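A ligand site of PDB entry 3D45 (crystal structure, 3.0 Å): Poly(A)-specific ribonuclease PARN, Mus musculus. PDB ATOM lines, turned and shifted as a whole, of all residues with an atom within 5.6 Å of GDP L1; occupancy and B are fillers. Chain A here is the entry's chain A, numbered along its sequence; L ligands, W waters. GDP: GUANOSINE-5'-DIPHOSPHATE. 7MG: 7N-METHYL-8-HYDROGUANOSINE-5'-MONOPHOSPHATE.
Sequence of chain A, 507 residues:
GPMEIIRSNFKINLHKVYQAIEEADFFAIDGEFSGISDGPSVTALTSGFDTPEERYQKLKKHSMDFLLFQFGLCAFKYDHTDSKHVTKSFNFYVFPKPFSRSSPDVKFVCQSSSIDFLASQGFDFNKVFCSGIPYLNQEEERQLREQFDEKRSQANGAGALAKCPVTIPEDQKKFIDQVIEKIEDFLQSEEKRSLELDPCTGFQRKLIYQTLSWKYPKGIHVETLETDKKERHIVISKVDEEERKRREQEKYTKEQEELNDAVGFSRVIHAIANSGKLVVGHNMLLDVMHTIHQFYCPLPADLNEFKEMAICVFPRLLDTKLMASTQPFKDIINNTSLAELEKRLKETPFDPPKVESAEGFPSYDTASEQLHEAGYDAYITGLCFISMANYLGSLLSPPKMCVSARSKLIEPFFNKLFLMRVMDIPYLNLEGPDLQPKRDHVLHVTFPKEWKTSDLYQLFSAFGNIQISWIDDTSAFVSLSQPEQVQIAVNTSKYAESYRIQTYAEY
SD of Met 420 lies within hydrogen-bond range of NH2 of Arg 421, 3.1 Å away. The side-chain sulfur (SD) of Met 420 sits close to the side-chain amide nitrogen (ND2) of Asn 283, at 3.7 Å. N of Leu 338 sits at hydrogen-bond distance from NE2 of His 282 (3.3 Å). O of Thr 336 lies close to NE2 of His 282 (3.1 Å). The backbone NH (N) of Ser 337 sits close to the side-chain amide nitrogen (ND2) of Asn 335. The side-chain amino group (NZ) of Lys 321 lies within hydrogen-bond range of the backbone carbonyl oxygen (O) of Thr 336 (3.2 Å). ND1 of His 282 lies within hydrogen-bond range of N of Lys 321 (3.5 Å).
The backbone carbonyl oxygen of Thr 336 sits close to an oxygen (O2A) of GDP L1, 3.2 Å away. Merely in contact with GDP L1: Phe 33 (3.5 Å), Ile 36 (3.8 Å), Leu 285 (3.8 Å) and Leu 286 (3.6 Å). Hydrophobic or aromatic side chains that line GDP L1: Phe 33, Ile 36, His 282, Leu 285, Leu 286, Leu 338 and Met 420. Within 4 Å of GDP L1: Phe 33, Ile 36, His 282, Asn 283, Leu 285, Leu 286, Lys 321, Thr 336, Ser 337, Leu 338, Met 420 and Arg 421. The nearest printed residue that does not touch GDP L1 is Leu 59 (4.5 Å).
NE2 of His 282 is in hydrogen-bond range of O2A of GDP L1 (2.9 Å). NH2 of Arg 421 lies within hydrogen-bond range of O6 of GDP L1, at 3.4 Å. NZ of Lys 321 is in salt-bridge range of OP2 of 7MG L2, 3.3 Å away. O5' of GDP L1 lies within hydrogen-bond range of ND2 of Asn 283. OG of Ser 337 lies within hydrogen-bond range of O2B of GDP L1 (3.4 Å). SD of Met 420 sits close to N1 of GDP L1. O2A of GDP L1 lies within salt-bridge range of NZ of Lys 321, at 2.5 Å. An oxygen (O1A) of GDP L1 sits at hydrogen-bond distance from the backbone NH of Leu 338, at 3.3 Å.
Water W3 lies within hydrogen-bond range of an oxygen (O1A) of GDP L1 (2.5 Å) and the backbone NH (N) of Leu 338 (3.1 Å). Water W4 lies within hydrogen-bond range of the side-chain carboxylate of Asp 30 (2.6 Å) and an oxygen (O3') of GDP L1 (3.0 Å). Water W1 lies within hydrogen-bond range of OD1 of Asn 283 (2.4 Å), O of Phe 418 (2.9 Å), N2 of GDP L1 (3.2 Å) and N of Leu 285 (3.2 Å). Water W2 lies within hydrogen-bond range of a nitrogen (N1) of GDP L1 (3.2 Å) and the backbone NH (N) of Met 420 (3.3 Å).
An oxygen (O2B) of GDP L1 lies close to an oxygen (O5') of 7MG L2.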
ATOM      1  N   ASP A  30       1.574  24.177   4.794  1.00  0.00           N
ATOM      2  CA  ASP A  30       1.507  22.718   4.905  1.00  0.00           C
ATOM      3  C   ASP A  30       1.371  22.075   3.551  1.00  0.00           C
ATOM      4  O   ASP A  30       0.763  22.656   2.638  1.00  0.00           O
ATOM      5  CB  ASP A  30       0.359  22.252   5.796  1.00  0.00           C
ATOM      6  CG  ASP A  30       0.440  20.784   6.074  1.00  0.00           C
ATOM      7  OD1 ASP A  30       1.608  20.299   6.137  1.00  0.00           O
ATOM      8  OD2 ASP A  30      -0.621  20.119   6.200  1.00  0.00           O
ATOM      9  N   GLY A  31       1.942  20.890   3.413  1.00  0.00           N
ATOM     10  CA  GLY A  31       1.843  20.161   2.163  1.00  0.00           C
ATOM     11  C   GLY A  31       1.088  18.862   2.328  1.00  0.00           C
ATOM     12  O   GLY A  31       1.217  18.208   3.358  1.00  0.00           O
ATOM     13  N   PHE A  33       0.973  15.257   0.174  1.00  0.00           N
ATOM     14  CA  PHE A  33       1.860  14.543  -0.737  1.00  0.00           C
ATOM     15  C   PHE A  33       1.207  13.311  -1.370  1.00  0.00           C
ATOM     16  O   PHE A  33       0.249  12.736  -0.844  1.00  0.00           O
ATOM     17  CB  PHE A  33       3.145  14.075  -0.029  1.00  0.00           C
ATOM     18  CG  PHE A  33       3.710  15.036   0.979  1.00  0.00           C
ATOM     19  CD1 PHE A  33       4.099  14.585   2.222  1.00  0.00           C
ATOM     20  CD2 PHE A  33       3.878  16.384   0.684  1.00  0.00           C
ATOM     21  CE1 PHE A  33       4.624  15.439   3.167  1.00  0.00           C
ATOM     22  CE2 PHE A  33       4.393  17.248   1.629  1.00  0.00           C
ATOM     23  CZ  PHE A  33       4.773  16.778   2.863  1.00  0.00           C
ATOM     24  N   ILE A  36       4.501   8.768   1.278  1.00  0.00           N
ATOM     25  CA  ILE A  36       5.602   8.997   2.243  1.00  0.00           C
ATOM     26  C   ILE A  36       6.864   8.209   1.939  1.00  0.00           C
ATOM     27  O   ILE A  36       7.938   8.808   1.727  1.00  0.00           O
ATOM     28  CB  ILE A  36       5.141   8.790   3.707  1.00  0.00           C
ATOM     29  CG1 ILE A  36       3.877   9.617   3.991  1.00  0.00           C
ATOM     30  CG2 ILE A  36       6.233   9.149   4.693  1.00  0.00           C
ATOM     31  CD1 ILE A  36       4.117  10.944   4.690  1.00  0.00           C
ATOM     32  N   LEU A  59      15.688  10.029   3.398  1.00  0.00           N
ATOM     33  CA  LEU A  59      14.526  10.782   2.955  1.00  0.00           C
ATOM     34  C   LEU A  59      14.741  11.293   1.530  1.00  0.00           C
ATOM     35  O   LEU A  59      13.793  11.391   0.744  1.00  0.00           O
ATOM     36  CB  LEU A  59      14.220  11.925   3.932  1.00  0.00           C
ATOM     37  CG  LEU A  59      14.051  11.459   5.388  1.00  0.00           C
ATOM     38  CD1 LEU A  59      13.605  12.552   6.334  1.00  0.00           C
ATOM     39  CD2 LEU A  59      13.088  10.284   5.474  1.00  0.00           C
ATOM     40  N   HIS A 282       4.358  22.468  10.738  1.00  0.00           N
ATOM     41  CA  HIS A 282       4.294  21.499  11.825  1.00  0.00           C
ATOM     42  C   HIS A 282       4.911  20.169  11.439  1.00  0.00           C
ATOM     43  O   HIS A 282       4.337  19.431  10.642  1.00  0.00           O
ATOM     44  CB  HIS A 282       2.856  21.257  12.302  1.00  0.00           C
ATOM     45  CG  HIS A 282       2.748  20.205  13.379  1.00  0.00           C
ATOM     46  ND1 HIS A 282       2.825  20.508  14.725  1.00  0.00           N
ATOM     47  CD2 HIS A 282       2.589  18.859  13.300  1.00  0.00           C
ATOM     48  CE1 HIS A 282       2.692  19.403  15.429  1.00  0.00           C
ATOM     49  NE2 HIS A 282       2.556  18.384  14.586  1.00  0.00           N
ATOM     50  N   ASN A 283       6.056  19.834  12.048  1.00  0.00           N
ATOM     51  CA  ASN A 283       6.831  18.640  11.685  1.00  0.00           C
ATOM     52  C   ASN A 283       7.133  18.660  10.190  1.00  0.00           C
ATOM     53  O   ASN A 283       6.853  17.693   9.484  1.00  0.00           O
ATOM     54  CB  ASN A 283       6.080  17.378  12.053  1.00  0.00           C
ATOM     55  CG  ASN A 283       6.960  16.150  11.989  1.00  0.00           C
ATOM     56  OD1 ASN A 283       8.084  16.218  11.514  1.00  0.00           O
ATOM     57  ND2 ASN A 283       6.466  15.029  12.504  1.00  0.00           N
ATOM     58  N   LEU A 285       9.930  18.954   8.053  1.00  0.00           N
ATOM     59  CA  LEU A 285      11.124  18.531   7.291  1.00  0.00           C
ATOM     60  C   LEU A 285      10.769  18.021   5.891  1.00  0.00           C
ATOM     61  O   LEU A 285      11.403  18.427   4.921  1.00  0.00           O
ATOM     62  CB  LEU A 285      11.972  17.504   8.055  1.00  0.00           C
ATOM     63  CG  LEU A 285      13.438  17.193   7.623  1.00  0.00           C
ATOM     64  CD1 LEU A 285      13.661  15.706   7.329  1.00  0.00           C
ATOM     65  CD2 LEU A 285      14.069  18.090   6.483  1.00  0.00           C
ATOM     66  N   LEU A 286       9.729  17.187   5.775  1.00  0.00           N
ATOM     67  CA  LEU A 286       9.246  16.777   4.436  1.00  0.00           C
ATOM     68  C   LEU A 286       8.648  17.926   3.597  1.00  0.00           C
ATOM     69  O   LEU A 286       8.974  18.070   2.421  1.00  0.00           O
ATOM     70  CB  LEU A 286       8.263  15.613   4.486  1.00  0.00           C
ATOM     71  CG  LEU A 286       8.766  14.315   5.129  1.00  0.00           C
ATOM     72  CD1 LEU A 286       7.668  13.277   5.165  1.00  0.00           C
ATOM     73  CD2 LEU A 286       9.959  13.762   4.376  1.00  0.00           C
ATOM     74  N   ASP A 287       7.788  18.748   4.199  1.00  0.00           N
ATOM     75  CA  ASP A 287       7.199  19.862   3.462  1.00  0.00           C
ATOM     76  C   ASP A 287       8.299  20.691   2.863  1.00  0.00           C
ATOM     77  O   ASP A 287       8.220  21.030   1.680  1.00  0.00           O
ATOM     78  CB  ASP A 287       6.341  20.746   4.344  1.00  0.00           C
ATOM     79  CG  ASP A 287       5.224  20.000   4.978  1.00  0.00           C
ATOM     80  OD1 ASP A 287       4.332  19.562   4.218  1.00  0.00           O
ATOM     81  OD2 ASP A 287       5.234  19.850   6.217  1.00  0.00           O
ATOM     82  N   LYS A 321       5.810  21.800  15.997  1.00  0.00           N
ATOM     83  CA  LYS A 321       6.016  20.554  16.696  1.00  0.00           C
ATOM     84  C   LYS A 321       7.297  20.586  17.548  1.00  0.00           C
ATOM     85  O   LYS A 321       7.358  19.953  18.597  1.00  0.00           O
ATOM     86  CB  LYS A 321       6.034  19.404  15.700  1.00  0.00           C
ATOM     87  CG  LYS A 321       6.353  18.044  16.283  1.00  0.00           C
ATOM     88  CD  LYS A 321       6.193  16.959  15.230  1.00  0.00           C
ATOM     89  CE  LYS A 321       6.143  15.579  15.852  1.00  0.00           C
ATOM     90  NZ  LYS A 321       4.793  15.223  16.362  1.00  0.00           N
ATOM     91  N   ASN A 335       1.319  15.093  24.061  1.00  0.00           N
ATOM     92  CA  ASN A 335       1.218  14.627  22.694  1.00  0.00           C
ATOM     93  C   ASN A 335       1.302  15.792  21.716  1.00  0.00           C
ATOM     94  O   ASN A 335       0.570  16.776  21.863  1.00  0.00           O
ATOM     95  CB  ASN A 335      -0.045  13.832  22.462  1.00  0.00           C
ATOM     96  CG  ASN A 335      -0.167  13.396  21.032  1.00  0.00           C
ATOM     97  OD1 ASN A 335       0.439  12.416  20.612  1.00  0.00           O
ATOM     98  ND2 ASN A 335      -0.907  14.162  20.242  1.00  0.00           N
ATOM     99  N   THR A 336       2.184  15.666  20.726  1.00  0.00           N
ATOM    100  CA  THR A 336       2.426  16.787  19.806  1.00  0.00           C
ATOM    101  C   THR A 336       1.971  16.558  18.375  1.00  0.00           C
ATOM    102  O   THR A 336       2.475  17.181  17.463  1.00  0.00           O
ATOM    103  CB  THR A 336       3.890  17.288  19.842  1.00  0.00           C
ATOM    104  OG1 THR A 336       4.774  16.255  19.427  1.00  0.00           O
ATOM    105  CG2 THR A 336       4.278  17.692  21.215  1.00  0.00           C
ATOM    106  N   SER A 337       1.024  15.638  18.180  1.00  0.00           N
ATOM    107  CA  SER A 337       0.235  15.540  16.942  1.00  0.00           C
ATOM    108  C   SER A 337      -0.403  16.888  16.750  1.00  0.00           C
ATOM    109  O   SER A 337      -0.870  17.500  17.706  1.00  0.00           O
ATOM    110  CB  SER A 337      -0.940  14.551  17.070  1.00  0.00           C
ATOM    111  OG  SER A 337      -0.518  13.218  17.219  1.00  0.00           O
ATOM    112  N   LEU A 338      -0.470  17.341  15.513  1.00  0.00           N
ATOM    113  CA  LEU A 338      -1.126  18.603  15.262  1.00  0.00           C
ATOM    114  C   LEU A 338      -2.541  18.620  15.850  1.00  0.00           C
ATOM    115  O   LEU A 338      -2.895  19.533  16.596  1.00  0.00           O
ATOM    116  CB  LEU A 338      -1.110  18.957  13.771  1.00  0.00           C
ATOM    117  CG  LEU A 338      -1.789  20.270  13.398  1.00  0.00           C
ATOM    118  CD1 LEU A 338      -1.345  21.404  14.317  1.00  0.00           C
ATOM    119  CD2 LEU A 338      -1.552  20.634  11.939  1.00  0.00           C
ATOM    120  N   ALA A 339      -3.338  17.594  15.555  1.00  0.00           N
ATOM    121  CA  ALA A 339      -4.706  17.489  16.104  1.00  0.00           C
ATOM    122  C   ALA A 339      -4.795  17.600  17.648  1.00  0.00           C
ATOM    123  O   ALA A 339      -5.630  18.348  18.189  1.00  0.00           O
ATOM    124  CB  ALA A 339      -5.377  16.204  15.623  1.00  0.00           C
ATOM    125  N   PHE A 418      12.213  19.979  12.902  1.00  0.00           N
ATOM    126  CA  PHE A 418      11.934  18.842  13.770  1.00  0.00           C
ATOM    127  C   PHE A 418      12.593  17.556  13.290  1.00  0.00           C
ATOM    128  O   PHE A 418      12.802  17.384  12.096  1.00  0.00           O
ATOM    129  CB  PHE A 418      10.438  18.583  13.888  1.00  0.00           C
ATOM    130  CG  PHE A 418      10.111  17.603  14.941  1.00  0.00           C
ATOM    131  CD1 PHE A 418      10.191  17.969  16.288  1.00  0.00           C
ATOM    132  CD2 PHE A 418       9.771  16.294  14.605  1.00  0.00           C
ATOM    133  CE1 PHE A 418       9.918  17.054  17.282  1.00  0.00           C
ATOM    134  CE2 PHE A 418       9.510  15.382  15.593  1.00  0.00           C
ATOM    135  CZ  PHE A 418       9.580  15.768  16.944  1.00  0.00           C
ATOM    136  N   LEU A 419      12.877  16.631  14.207  1.00  0.00           N
ATOM    137  CA  LEU A 419      13.419  15.346  13.801  1.00  0.00           C
ATOM    138  C   LEU A 419      12.557  14.158  14.305  1.00  0.00           C
ATOM    139  O   LEU A 419      12.067  14.182  15.431  1.00  0.00           O
ATOM    140  CB  LEU A 419      14.886  15.258  14.227  1.00  0.00           C
ATOM    141  CG  LEU A 419      15.819  14.927  13.068  1.00  0.00           C
ATOM    142  CD1 LEU A 419      15.070  15.012  11.764  1.00  0.00           C
ATOM    143  CD2 LEU A 419      16.977  15.826  13.046  1.00  0.00           C
ATOM    144  N   MET A 420      12.338  13.147  13.459  1.00  0.00           N
ATOM    145  CA  MET A 420      11.590  11.965  13.902  1.00  0.00           C
ATOM    146  C   MET A 420      12.476  10.749  14.267  1.00  0.00           C
ATOM    147  O   MET A 420      13.602  10.571  13.737  1.00  0.00           O
ATOM    148  CB  MET A 420      10.522  11.581  12.870  1.00  0.00           C
ATOM    149  CG  MET A 420       9.129  11.946  13.280  1.00  0.00           C
ATOM    150  SD  MET A 420       7.915  11.664  11.992  1.00  0.00           S
ATOM    151  CE  MET A 420       6.413  11.642  12.961  1.00  0.00           C
ATOM    152  N   ARG A 421      11.999   9.912  15.189  1.00  0.00           N
ATOM    153  CA  ARG A 421      12.585   8.593  15.351  1.00  0.00           C
ATOM    154  C   ARG A 421      14.093   8.629  15.391  1.00  0.00           C
ATOM    155  O   ARG A 421      14.746   7.937  14.600  1.00  0.00           O
ATOM    156  CB  ARG A 421      12.195   7.713  14.164  1.00  0.00           C
ATOM    157  CG  ARG A 421      10.975   6.867  14.362  1.00  0.00           C
ATOM    158  CD  ARG A 421      10.593   6.227  13.062  1.00  0.00           C
ATOM    159  NE  ARG A 421      10.098   7.261  12.171  1.00  0.00           N
ATOM    160  CZ  ARG A 421       8.870   7.762  12.238  1.00  0.00           C
ATOM    161  NH1 ARG A 421       8.009   7.322  13.155  1.00  0.00           N
ATOM    162  NH2 ARG A 421       8.513   8.712  11.395  1.00  0.00           N
HETATM  163  PB  GDP L   1       2.906  12.322  14.382  1.00  0.00           P
HETATM  164  O1B GDP L   1       3.359  11.234  13.450  1.00  0.00           O
HETATM  165  O2B GDP L   1       2.038  11.720  15.460  1.00  0.00           O
HETATM  166  O3B GDP L   1       4.149  13.007  14.900  1.00  0.00           O
HETATM  167  O3A GDP L   1       1.962  13.372  13.627  1.00  0.00           O
HETATM  168  PA  GDP L   1       2.314  14.937  13.526  1.00  0.00           P
HETATM  169  O1A GDP L   1       1.058  15.677  13.080  1.00  0.00           O
HETATM  170  O2A GDP L   1       2.930  15.523  14.771  1.00  0.00           O
HETATM  171  O5' GDP L   1       3.345  14.857  12.300  1.00  0.00           O
HETATM  172  C5' GDP L   1       2.898  14.188  11.135  1.00  0.00           C
HETATM  173  C4' GDP L   1       3.530  14.789   9.902  1.00  0.00           C
HETATM  174  O4' GDP L   1       4.884  14.365   9.814  1.00  0.00           O
HETATM  175  C3' GDP L   1       2.838  14.258   8.674  1.00  0.00           C
HETATM  176  O3' GDP L   1       2.063  15.329   8.160  1.00  0.00           O
HETATM  177  C2' GDP L   1       3.933  13.822   7.719  1.00  0.00           C
HETATM  178  O2' GDP L   1       3.969  14.645   6.559  1.00  0.00           O
HETATM  179  C1' GDP L   1       5.223  14.037   8.473  1.00  0.00           C
HETATM  180  N9  GDP L   1       6.099  12.834   8.428  1.00  0.00           N
HETATM  181  C8  GDP L   1       5.748  11.564   8.102  1.00  0.00           C
HETATM  182  N7  GDP L   1       6.809  10.724   8.137  1.00  0.00           N
HETATM  183  C5  GDP L   1       7.871  11.453   8.501  1.00  0.00           C
HETATM  184  C6  GDP L   1       9.316  11.210   8.730  1.00  0.00           C
HETATM  185  O6  GDP L   1       9.793  10.080   8.603  1.00  0.00           O
HETATM  186  N1  GDP L   1      10.101  12.222   9.095  1.00  0.00           N
HETATM  187  C2  GDP L   1       9.601  13.457   9.252  1.00  0.00           C
HETATM  188  N2  GDP L   1      10.464  14.428   9.627  1.00  0.00           N
HETATM  189  N3  GDP L   1       8.298  13.772   9.050  1.00  0.00           N
HETATM  190  C4  GDP L   1       7.402  12.838   8.689  1.00  0.00           C
HETATM  191  P   7MG L   2       4.164  11.873  17.033  1.00  0.00           P
HETATM  192  OP1 7MG L   2       3.053  11.881  18.028  1.00  0.00           O
HETATM  193  OP2 7MG L   2       5.584  12.132  17.368  1.00  0.00           O
HETATM  194  O5' 7MG L   2       4.193  10.476  16.296  1.00  0.00           O
HETATM  195  C5' 7MG L   2       5.020   9.592  16.950  1.00  0.00           C
HETATM  196  C4' 7MG L   2       4.709   8.162  16.602  1.00  0.00           C
HETATM  197  O4' 7MG L   2       4.834   7.408  17.829  1.00  0.00           O
HETATM  198  C3' 7MG L   2       3.359   7.834  15.987  1.00  0.00           C
HETATM  199  O3' 7MG L   2       3.621   6.877  15.018  1.00  0.00           O
HETATM  200  C2' 7MG L   2       2.575   7.145  17.084  1.00  0.00           C
HETATM  201  O2' 7MG L   2       2.155   5.857  16.707  1.00  0.00           O
HETATM  202  C1' 7MG L   2       3.572   6.935  18.202  1.00  0.00           C
HETATM  203  N9  7MG L   2       3.084   7.559  19.400  1.00  0.00           N
HETATM  204  C8  7MG L   2       2.921   8.897  19.672  1.00  0.00           C
HETATM  205  N7  7MG L   2       2.399   9.067  20.862  1.00  0.00           N
HETATM  206  C5  7MG L   2       2.226   7.778  21.355  1.00  0.00           C
HETATM  207  C6  7MG L   2       1.704   7.368  22.571  1.00  0.00           C
HETATM  208  O6  7MG L   2       1.283   8.077  23.499  1.00  0.00           O
HETATM  209  N1  7MG L   2       1.705   5.975  22.683  1.00  0.00           N
HETATM  210  C2  7MG L   2       2.141   5.082  21.738  1.00  0.00           C
HETATM  211  N2  7MG L   2       2.047   3.767  22.069  1.00  0.00           N
HETATM  212  N3  7MG L   2       2.629   5.487  20.564  1.00  0.00           N
HETATM  213  C4  7MG L   2       2.633   6.844  20.464  1.00  0.00           C
HETATM  214  CM7 7MG L   2       2.131  10.305  21.597  1.00  0.00           C
HETATM  215  O   HOH W   1      10.149  17.323  10.829  1.00  0.00           O
HETATM  216  O   HOH W   2      13.015  12.445  10.327  1.00  0.00           O
HETATM  217  O   HOH W   3      -1.356  15.088  13.569  1.00  0.00           O
HETATM  218  O   HOH W   4       1.810  18.335   7.877  1.00  0.00           O
